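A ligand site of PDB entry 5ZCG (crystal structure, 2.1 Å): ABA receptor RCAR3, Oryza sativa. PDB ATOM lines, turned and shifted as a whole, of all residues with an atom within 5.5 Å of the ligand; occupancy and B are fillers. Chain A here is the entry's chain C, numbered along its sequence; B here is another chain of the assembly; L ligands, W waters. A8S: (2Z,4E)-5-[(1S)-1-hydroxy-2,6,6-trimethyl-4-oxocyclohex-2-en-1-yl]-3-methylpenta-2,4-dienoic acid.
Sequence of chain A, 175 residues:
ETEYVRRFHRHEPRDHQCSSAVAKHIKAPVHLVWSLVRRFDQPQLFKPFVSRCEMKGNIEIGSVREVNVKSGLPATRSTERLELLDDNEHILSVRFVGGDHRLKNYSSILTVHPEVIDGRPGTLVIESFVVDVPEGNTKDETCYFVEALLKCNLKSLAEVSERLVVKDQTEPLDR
An oxygen (O11) of the ligand sits at hydrogen-bond distance from the side-chain amide nitrogen (ND2) of Asn 153 (2.9 Å).
The side-chain amino group (NZ) of Lys 47 is in salt-bridge range of an oxygen (O12) of the ligand (3.0 Å).
The backbone NH (N) of Phe 96 lies within hydrogen-bond range of the backbone carbonyl oxygen (O) of Tyr 106, 2.8 Å away.
The backbone NH of Leu 103 sits at hydrogen-bond distance from a ring nitrogen (ND1) of His 101 (3.2 Å).
OG of Ser 78 sits at hydrogen-bond distance from NE2 of His 101 (3.2 Å).
The side-chain carboxylate (OE1) of Glu 80 sits at hydrogen-bond distance from the side-chain hydroxyl (OG) of Ser 78.
The backbone NH (N) of Val 69 is in hydrogen-bond range of the backbone carbonyl oxygen (O) of Thr 76.
Water W3 lies within hydrogen-bond range of an oxygen (O12) of the ligand (2.6 Å), the side-chain carboxylate of Glu 127 (2.6 Å), the side-chain hydroxyl of Tyr 106 (2.7 Å) and the side-chain hydroxyl of Ser 108 (3.1 Å).
Water W2 bridges OE1 of Glu 80 (2.5 Å) and O7 of the ligand (2.6 Å).
CB of Phe 49 touches C13 of the ligand (3.8 Å).
CG1 of Val 69 touches O7 of the ligand, at 3.9 Å.
Leu 73 touches the ligand (CD1 to C13, 3.8 Å).
CD of Pro 74 touches O10 of the ligand, at 3.9 Å.
Ala 75 touches the ligand (CB to O10, 3.7 Å).
Ser 78 touches the ligand.
Phe 96 touches the ligand (CE2 to C15, 3.5 Å).
His 101 touches the ligand.
Leu 103 touches the ligand (CD1 to C6, 3.6 Å).
Tyr 106 touches the ligand (OH to C2, 3.8 Å).
Phe 145 touches the ligand.
Leu 149 touches the ligand.
CD2 of Leu 150 touches C2 of the ligand (3.7 Å).
Within 4 Å of the ligand: Lys 47, Phe 49, Val 69, Leu 73, Pro 74, Ala 75, Ser 78, Phe 96, His 101, Leu 103, Tyr 106, Phe 145, Leu 149, Leu 150 and Asn 153.
The nearest printed residue that does not touch the ligand is Arg 77 (4.1 Å).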
ATOM      1  N   LYS A  47      13.046 -12.110 -31.275  1.00  0.00           N
ATOM      2  CA  LYS A  47      13.578 -11.552 -30.031  1.00  0.00           C
ATOM      3  C   LYS A  47      14.846 -10.755 -30.335  1.00  0.00           C
ATOM      4  O   LYS A  47      15.866 -11.347 -30.729  1.00  0.00           O
ATOM      5  CB  LYS A  47      13.864 -12.650 -29.010  1.00  0.00           C
ATOM      6  CG  LYS A  47      12.609 -13.329 -28.491  1.00  0.00           C
ATOM      7  CD  LYS A  47      12.799 -13.812 -27.069  1.00  0.00           C
ATOM      8  CE  LYS A  47      11.620 -14.645 -26.609  1.00  0.00           C
ATOM      9  NZ  LYS A  47      11.888 -15.247 -25.282  1.00  0.00           N
ATOM     10  N   PHE A  49      17.121  -9.257 -28.600  1.00  0.00           N
ATOM     11  CA  PHE A  49      18.297  -9.343 -27.744  1.00  0.00           C
ATOM     12  C   PHE A  49      19.037 -10.664 -27.859  1.00  0.00           C
ATOM     13  O   PHE A  49      20.129 -10.791 -27.304  1.00  0.00           O
ATOM     14  CB  PHE A  49      17.910  -9.099 -26.281  1.00  0.00           C
ATOM     15  CG  PHE A  49      17.373  -7.718 -26.021  1.00  0.00           C
ATOM     16  CD1 PHE A  49      18.222  -6.629 -26.021  1.00  0.00           C
ATOM     17  CD2 PHE A  49      16.024  -7.516 -25.790  1.00  0.00           C
ATOM     18  CE1 PHE A  49      17.743  -5.344 -25.780  1.00  0.00           C
ATOM     19  CE2 PHE A  49      15.532  -6.234 -25.556  1.00  0.00           C
ATOM     20  CZ  PHE A  49      16.391  -5.155 -25.553  1.00  0.00           C
ATOM     21  N   VAL A  69      22.649 -13.728 -25.136  1.00  0.00           N
ATOM     22  CA  VAL A  69      22.083 -12.451 -25.497  1.00  0.00           C
ATOM     23  C   VAL A  69      23.213 -11.510 -25.911  1.00  0.00           C
ATOM     24  O   VAL A  69      24.397 -11.769 -25.670  1.00  0.00           O
ATOM     25  CB  VAL A  69      21.232 -11.838 -24.354  1.00  0.00           C
ATOM     26  CG1 VAL A  69      19.990 -12.689 -24.106  1.00  0.00           C
ATOM     27  CG2 VAL A  69      22.057 -11.685 -23.084  1.00  0.00           C
ATOM     28  N   LEU A  73      23.634  -5.756 -21.883  1.00  0.00           N
ATOM     29  CA  LEU A  73      22.537  -6.200 -21.028  1.00  0.00           C
ATOM     30  C   LEU A  73      23.033  -6.573 -19.630  1.00  0.00           C
ATOM     31  O   LEU A  73      24.230  -6.777 -19.421  1.00  0.00           O
ATOM     32  CB  LEU A  73      21.817  -7.375 -21.676  1.00  0.00           C
ATOM     33  CG  LEU A  73      21.012  -7.055 -22.931  1.00  0.00           C
ATOM     34  CD1 LEU A  73      20.496  -8.322 -23.587  1.00  0.00           C
ATOM     35  CD2 LEU A  73      19.862  -6.125 -22.596  1.00  0.00           C
ATOM     36  N   PRO A  74      22.127  -6.678 -18.651  1.00  0.00           N
ATOM     37  CA  PRO A  74      22.552  -7.088 -17.303  1.00  0.00           C
ATOM     38  C   PRO A  74      23.050  -8.525 -17.222  1.00  0.00           C
ATOM     39  O   PRO A  74      23.658  -8.886 -16.208  1.00  0.00           O
ATOM     40  CB  PRO A  74      21.274  -6.918 -16.455  1.00  0.00           C
ATOM     41  CG  PRO A  74      20.418  -5.988 -17.238  1.00  0.00           C
ATOM     42  CD  PRO A  74      20.715  -6.262 -18.673  1.00  0.00           C
ATOM     43  N   ALA A  75      22.825  -9.344 -18.249  1.00  0.00           N
ATOM     44  CA  ALA A  75      23.233 -10.743 -18.246  1.00  0.00           C
ATOM     45  C   ALA A  75      23.732 -11.123 -19.628  1.00  0.00           C
ATOM     46  O   ALA A  75      23.632 -10.348 -20.578  1.00  0.00           O
ATOM     47  CB  ALA A  75      22.073 -11.665 -17.827  1.00  0.00           C
ATOM     48  N   THR A  76      24.256 -12.342 -19.737  1.00  0.00           N
ATOM     49  CA  THR A  76      24.783 -12.832 -20.999  1.00  0.00           C
ATOM     50  C   THR A  76      24.106 -14.092 -21.524  1.00  0.00           C
ATOM     51  O   THR A  76      24.079 -14.284 -22.739  1.00  0.00           O
ATOM     52  CB  THR A  76      26.300 -13.121 -20.879  1.00  0.00           C
ATOM     53  OG1 THR A  76      26.521 -14.141 -19.907  1.00  0.00           O
ATOM     54  CG2 THR A  76      27.053 -11.848 -20.472  1.00  0.00           C
ATOM     55  N   ARG A  77      23.553 -14.931 -20.654  1.00  0.00           N
ATOM     56  CA  ARG A  77      23.032 -16.202 -21.129  1.00  0.00           C
ATOM     57  C   ARG A  77      21.826 -16.606 -20.301  1.00  0.00           C
ATOM     58  O   ARG A  77      21.590 -16.102 -19.189  1.00  0.00           O
ATOM     59  CB  ARG A  77      24.103 -17.298 -21.074  1.00  0.00           C
ATOM     60  CG  ARG A  77      24.745 -17.477 -19.698  1.00  0.00           C
ATOM     61  CD  ARG A  77      25.750 -18.613 -19.685  1.00  0.00           C
ATOM     62  NE  ARG A  77      26.227 -18.884 -18.326  1.00  0.00           N
ATOM     63  CZ  ARG A  77      25.651 -19.718 -17.479  1.00  0.00           C
ATOM     64  NH1 ARG A  77      24.549 -20.388 -17.818  1.00  0.00           N
ATOM     65  NH2 ARG A  77      26.158 -19.886 -16.269  1.00  0.00           N
ATOM     66  N   SER A  78      21.038 -17.526 -20.858  1.00  0.00           N
ATOM     67  CA  SER A  78      19.832 -18.010 -20.209  1.00  0.00           C
ATOM     68  C   SER A  78      19.570 -19.429 -20.690  1.00  0.00           C
ATOM     69  O   SER A  78      19.819 -19.760 -21.840  1.00  0.00           O
ATOM     70  CB  SER A  78      18.639 -17.109 -20.501  1.00  0.00           C
ATOM     71  OG  SER A  78      17.542 -17.435 -19.653  1.00  0.00           O
ATOM     72  N   GLU A  80      16.439 -22.176 -20.837  1.00  0.00           N
ATOM     73  CA  GLU A  80      14.997 -21.967 -20.864  1.00  0.00           C
ATOM     74  C   GLU A  80      14.305 -23.258 -21.254  1.00  0.00           C
ATOM     75  O   GLU A  80      14.680 -23.904 -22.242  1.00  0.00           O
ATOM     76  CB  GLU A  80      14.658 -20.832 -21.834  1.00  0.00           C
ATOM     77  CG  GLU A  80      15.230 -19.488 -21.380  1.00  0.00           C
ATOM     78  CD  GLU A  80      15.193 -18.386 -22.441  1.00  0.00           C
ATOM     79  OE1 GLU A  80      15.757 -17.305 -22.162  1.00  0.00           O
ATOM     80  OE2 GLU A  80      14.637 -18.588 -23.533  1.00  0.00           O
ATOM     81  N   PHE A  96      12.553 -20.082 -17.035  1.00  0.00           N
ATOM     82  CA  PHE A  96      13.993 -19.876 -17.033  1.00  0.00           C
ATOM     83  C   PHE A  96      14.591 -20.797 -15.968  1.00  0.00           C
ATOM     84  O   PHE A  96      14.417 -20.553 -14.767  1.00  0.00           O
ATOM     85  CB  PHE A  96      14.345 -18.415 -16.755  1.00  0.00           C
ATOM     86  CG  PHE A  96      13.943 -17.459 -17.850  1.00  0.00           C
ATOM     87  CD1 PHE A  96      13.326 -17.907 -19.012  1.00  0.00           C
ATOM     88  CD2 PHE A  96      14.184 -16.100 -17.718  1.00  0.00           C
ATOM     89  CE1 PHE A  96      12.959 -17.031 -20.014  1.00  0.00           C
ATOM     90  CE2 PHE A  96      13.827 -15.204 -18.717  1.00  0.00           C
ATOM     91  CZ  PHE A  96      13.217 -15.672 -19.868  1.00  0.00           C
ATOM     92  N   HIS A 101      21.666 -14.537 -15.003  1.00  0.00           N
ATOM     93  CA  HIS A 101      20.827 -13.371 -14.787  1.00  0.00           C
ATOM     94  C   HIS A 101      20.200 -13.416 -13.391  1.00  0.00           C
ATOM     95  O   HIS A 101      20.465 -14.324 -12.584  1.00  0.00           O
ATOM     96  CB  HIS A 101      19.736 -13.300 -15.857  1.00  0.00           C
ATOM     97  CG  HIS A 101      18.989 -14.580 -16.040  1.00  0.00           C
ATOM     98  ND1 HIS A 101      17.994 -14.982 -15.165  1.00  0.00           N
ATOM     99  CD2 HIS A 101      19.079 -15.547 -16.980  1.00  0.00           C
ATOM    100  CE1 HIS A 101      17.516 -16.150 -15.566  1.00  0.00           C
ATOM    101  NE2 HIS A 101      18.154 -16.507 -16.666  1.00  0.00           N
ATOM    102  N   LEU A 103      16.746 -13.280 -12.791  1.00  0.00           N
ATOM    103  CA  LEU A 103      15.321 -13.573 -12.922  1.00  0.00           C
ATOM    104  C   LEU A 103      15.088 -15.033 -12.533  1.00  0.00           C
ATOM    105  O   LEU A 103      14.819 -15.901 -13.364  1.00  0.00           O
ATOM    106  CB  LEU A 103      14.856 -13.284 -14.355  1.00  0.00           C
ATOM    107  CG  LEU A 103      14.947 -11.835 -14.827  1.00  0.00           C
ATOM    108  CD1 LEU A 103      14.519 -11.710 -16.274  1.00  0.00           C
ATOM    109  CD2 LEU A 103      14.099 -10.919 -13.947  1.00  0.00           C
ATOM    110  N   TYR A 106      11.702 -17.526 -13.111  1.00  0.00           N
ATOM    111  CA  TYR A 106      10.895 -16.806 -14.079  1.00  0.00           C
ATOM    112  C   TYR A 106      10.098 -17.800 -14.910  1.00  0.00           C
ATOM    113  O   TYR A 106      10.634 -18.782 -15.422  1.00  0.00           O
ATOM    114  CB  TYR A 106      11.797 -15.964 -14.975  1.00  0.00           C
ATOM    115  CG  TYR A 106      11.096 -15.206 -16.081  1.00  0.00           C
ATOM    116  CD1 TYR A 106      10.737 -15.835 -17.264  1.00  0.00           C
ATOM    117  CD2 TYR A 106      10.798 -13.854 -15.934  1.00  0.00           C
ATOM    118  CE1 TYR A 106      10.097 -15.140 -18.273  1.00  0.00           C
ATOM    119  CE2 TYR A 106      10.166 -13.152 -16.944  1.00  0.00           C
ATOM    120  CZ  TYR A 106       9.814 -13.802 -18.116  1.00  0.00           C
ATOM    121  OH  TYR A 106       9.174 -13.106 -19.125  1.00  0.00           O
ATOM    122  N   SER A 108       6.832 -17.618 -17.935  1.00  0.00           N
ATOM    123  CA  SER A 108       6.043 -16.741 -18.774  1.00  0.00           C
ATOM    124  C   SER A 108       5.029 -17.552 -19.570  1.00  0.00           C
ATOM    125  O   SER A 108       5.279 -18.704 -19.947  1.00  0.00           O
ATOM    126  CB  SER A 108       6.917 -15.929 -19.743  1.00  0.00           C
ATOM    127  OG  SER A 108       7.312 -16.722 -20.841  1.00  0.00           O
ATOM    128  N   GLU A 127       1.472 -11.508 -23.156  1.00  0.00           N
ATOM    129  CA  GLU A 127       2.486 -12.252 -22.445  1.00  0.00           C
ATOM    130  C   GLU A 127       2.520 -11.797 -20.990  1.00  0.00           C
ATOM    131  O   GLU A 127       2.693 -10.606 -20.719  1.00  0.00           O
ATOM    132  CB  GLU A 127       3.870 -12.080 -23.090  1.00  0.00           C
ATOM    133  CG  GLU A 127       4.998 -12.755 -22.313  1.00  0.00           C
ATOM    134  CD  GLU A 127       6.139 -13.188 -23.205  1.00  0.00           C
ATOM    135  OE1 GLU A 127       6.266 -12.649 -24.324  1.00  0.00           O
ATOM    136  OE2 GLU A 127       6.919 -14.076 -22.788  1.00  0.00           O
ATOM    137  N   PHE A 145      11.317  -3.616 -15.305  1.00  0.00           N
ATOM    138  CA  PHE A 145      12.401  -4.150 -16.121  1.00  0.00           C
ATOM    139  C   PHE A 145      11.908  -5.232 -17.083  1.00  0.00           C
ATOM    140  O   PHE A 145      12.166  -5.182 -18.295  1.00  0.00           O
ATOM    141  CB  PHE A 145      13.490  -4.675 -15.170  1.00  0.00           C
ATOM    142  CG  PHE A 145      14.545  -5.505 -15.830  1.00  0.00           C
ATOM    143  CD1 PHE A 145      15.520  -4.931 -16.622  1.00  0.00           C
ATOM    144  CD2 PHE A 145      14.582  -6.879 -15.632  1.00  0.00           C
ATOM    145  CE1 PHE A 145      16.502  -5.701 -17.220  1.00  0.00           C
ATOM    146  CE2 PHE A 145      15.557  -7.656 -16.230  1.00  0.00           C
ATOM    147  CZ  PHE A 145      16.518  -7.065 -17.017  1.00  0.00           C
ATOM    148  N   VAL A 146      11.175  -6.210 -16.552  1.00  0.00           N
ATOM    149  CA  VAL A 146      10.693  -7.284 -17.415  1.00  0.00           C
ATOM    150  C   VAL A 146       9.753  -6.734 -18.473  1.00  0.00           C
ATOM    151  O   VAL A 146       9.784  -7.157 -19.633  1.00  0.00           O
ATOM    152  CB  VAL A 146      10.026  -8.394 -16.581  1.00  0.00           C
ATOM    153  CG1 VAL A 146       9.463  -9.465 -17.495  1.00  0.00           C
ATOM    154  CG2 VAL A 146      11.015  -8.997 -15.593  1.00  0.00           C
ATOM    155  N   LEU A 149      11.637  -5.177 -21.387  1.00  0.00           N
ATOM    156  CA  LEU A 149      12.188  -6.192 -22.295  1.00  0.00           C
ATOM    157  C   LEU A 149      11.093  -6.860 -23.124  1.00  0.00           C
ATOM    158  O   LEU A 149      11.228  -7.006 -24.342  1.00  0.00           O
ATOM    159  CB  LEU A 149      12.954  -7.243 -21.489  1.00  0.00           C
ATOM    160  CG  LEU A 149      14.215  -6.733 -20.778  1.00  0.00           C
ATOM    161  CD1 LEU A 149      14.852  -7.835 -19.954  1.00  0.00           C
ATOM    162  CD2 LEU A 149      15.206  -6.160 -21.785  1.00  0.00           C
ATOM    163  N   LEU A 150       9.989  -7.248 -22.480  1.00  0.00           N
ATOM    164  CA  LEU A 150       8.907  -7.920 -23.178  1.00  0.00           C
ATOM    165  C   LEU A 150       8.258  -7.012 -24.218  1.00  0.00           C
ATOM    166  O   LEU A 150       7.817  -7.482 -25.271  1.00  0.00           O
ATOM    167  CB  LEU A 150       7.855  -8.415 -22.185  1.00  0.00           C
ATOM    168  CG  LEU A 150       8.277  -9.580 -21.282  1.00  0.00           C
ATOM    169  CD1 LEU A 150       7.118 -10.008 -20.393  1.00  0.00           C
ATOM    170  CD2 LEU A 150       8.775 -10.733 -22.122  1.00  0.00           C
ATOM    171  N   ASN A 153      10.374  -7.147 -27.174  1.00  0.00           N
ATOM    172  CA  ASN A 153      10.181  -8.427 -27.860  1.00  0.00           C
ATOM    173  C   ASN A 153       8.905  -8.395 -28.705  1.00  0.00           C
ATOM    174  O   ASN A 153       8.909  -8.804 -29.867  1.00  0.00           O
ATOM    175  CB  ASN A 153      10.126  -9.575 -26.854  1.00  0.00           C
ATOM    176  CG  ASN A 153      11.490  -9.992 -26.342  1.00  0.00           C
ATOM    177  OD1 ASN A 153      12.525  -9.578 -26.854  1.00  0.00           O
ATOM    178  ND2 ASN A 153      11.496 -10.844 -25.319  1.00  0.00           N
ATOM    179  N   TRP B 202      20.380  -2.951 -11.262  1.00  0.00           N
ATOM    180  CA  TRP B 202      20.192  -4.328 -11.729  1.00  0.00           C
ATOM    181  C   TRP B 202      21.513  -4.744 -12.367  1.00  0.00           C
ATOM    182  O   TRP B 202      21.705  -4.560 -13.574  1.00  0.00           O
ATOM    183  CB  TRP B 202      19.038  -4.409 -12.706  1.00  0.00           C
ATOM    184  CG  TRP B 202      18.462  -5.773 -12.898  1.00  0.00           C
ATOM    185  CD1 TRP B 202      18.997  -6.784 -13.642  1.00  0.00           C
ATOM    186  CD2 TRP B 202      17.237  -6.271 -12.347  1.00  0.00           C
ATOM    187  NE1 TRP B 202      18.174  -7.890 -13.590  1.00  0.00           N
ATOM    188  CE2 TRP B 202      17.093  -7.602 -12.795  1.00  0.00           C
ATOM    189  CE3 TRP B 202      16.256  -5.725 -11.514  1.00  0.00           C
ATOM    190  CZ2 TRP B 202      16.003  -8.390 -12.445  1.00  0.00           C
ATOM    191  CZ3 TRP B 202      15.170  -6.519 -11.170  1.00  0.00           C
ATOM    192  CH2 TRP B 202      15.047  -7.833 -11.635  1.00  0.00           C
HETATM  193  C1  A8S L   1      12.146 -12.837 -22.638  1.00  0.00           C
HETATM  194  C2  A8S L   1      12.137 -12.063 -21.319  1.00  0.00           C
HETATM  195  C3  A8S L   1      13.224 -11.576 -20.702  1.00  0.00           C
HETATM  196  C4  A8S L   1      14.653 -11.723 -21.275  1.00  0.00           C
HETATM  197  C5  A8S L   1      15.780 -11.707 -20.480  1.00  0.00           C
HETATM  198  C6  A8S L   1      13.008 -10.831 -19.382  1.00  0.00           C
HETATM  199  C7  A8S L   1      17.205 -11.847 -21.112  1.00  0.00           C
HETATM  200  O7  A8S L   1      16.600 -12.649 -22.109  1.00  0.00           O
HETATM  201  C8  A8S L   1      17.166 -10.302 -21.211  1.00  0.00           C
HETATM  202  C9  A8S L   1      17.906  -9.523 -20.118  1.00  0.00           C
HETATM  203  C10 A8S L   1      18.294 -10.263 -18.832  1.00  0.00           C
HETATM  204  O10 A8S L   1      18.966  -9.732 -18.009  1.00  0.00           O
HETATM  205  C11 A8S L   1      17.826 -11.706 -18.594  1.00  0.00           C
HETATM  206  O11 A8S L   1      13.004 -12.616 -23.529  1.00  0.00           O
HETATM  207  C12 A8S L   1      17.722 -12.567 -19.845  1.00  0.00           C
HETATM  208  O12 A8S L   1      11.251 -13.692 -22.853  1.00  0.00           O
HETATM  209  C13 A8S L   1      17.091  -9.655 -22.599  1.00  0.00           C
HETATM  210  C14 A8S L   1      19.139 -13.028 -20.182  1.00  0.00           C
HETATM  211  C15 A8S L   1      16.890 -13.822 -19.529  1.00  0.00           C
HETATM  212  O   HOH W   1      15.436 -12.357 -24.828  1.00  0.00           O
HETATM  213  O   HOH W   2      15.998 -15.007 -23.105  1.00  0.00           O
HETATM  214  O   HOH W   3       9.169 -14.361 -21.463  1.00  0.00           O
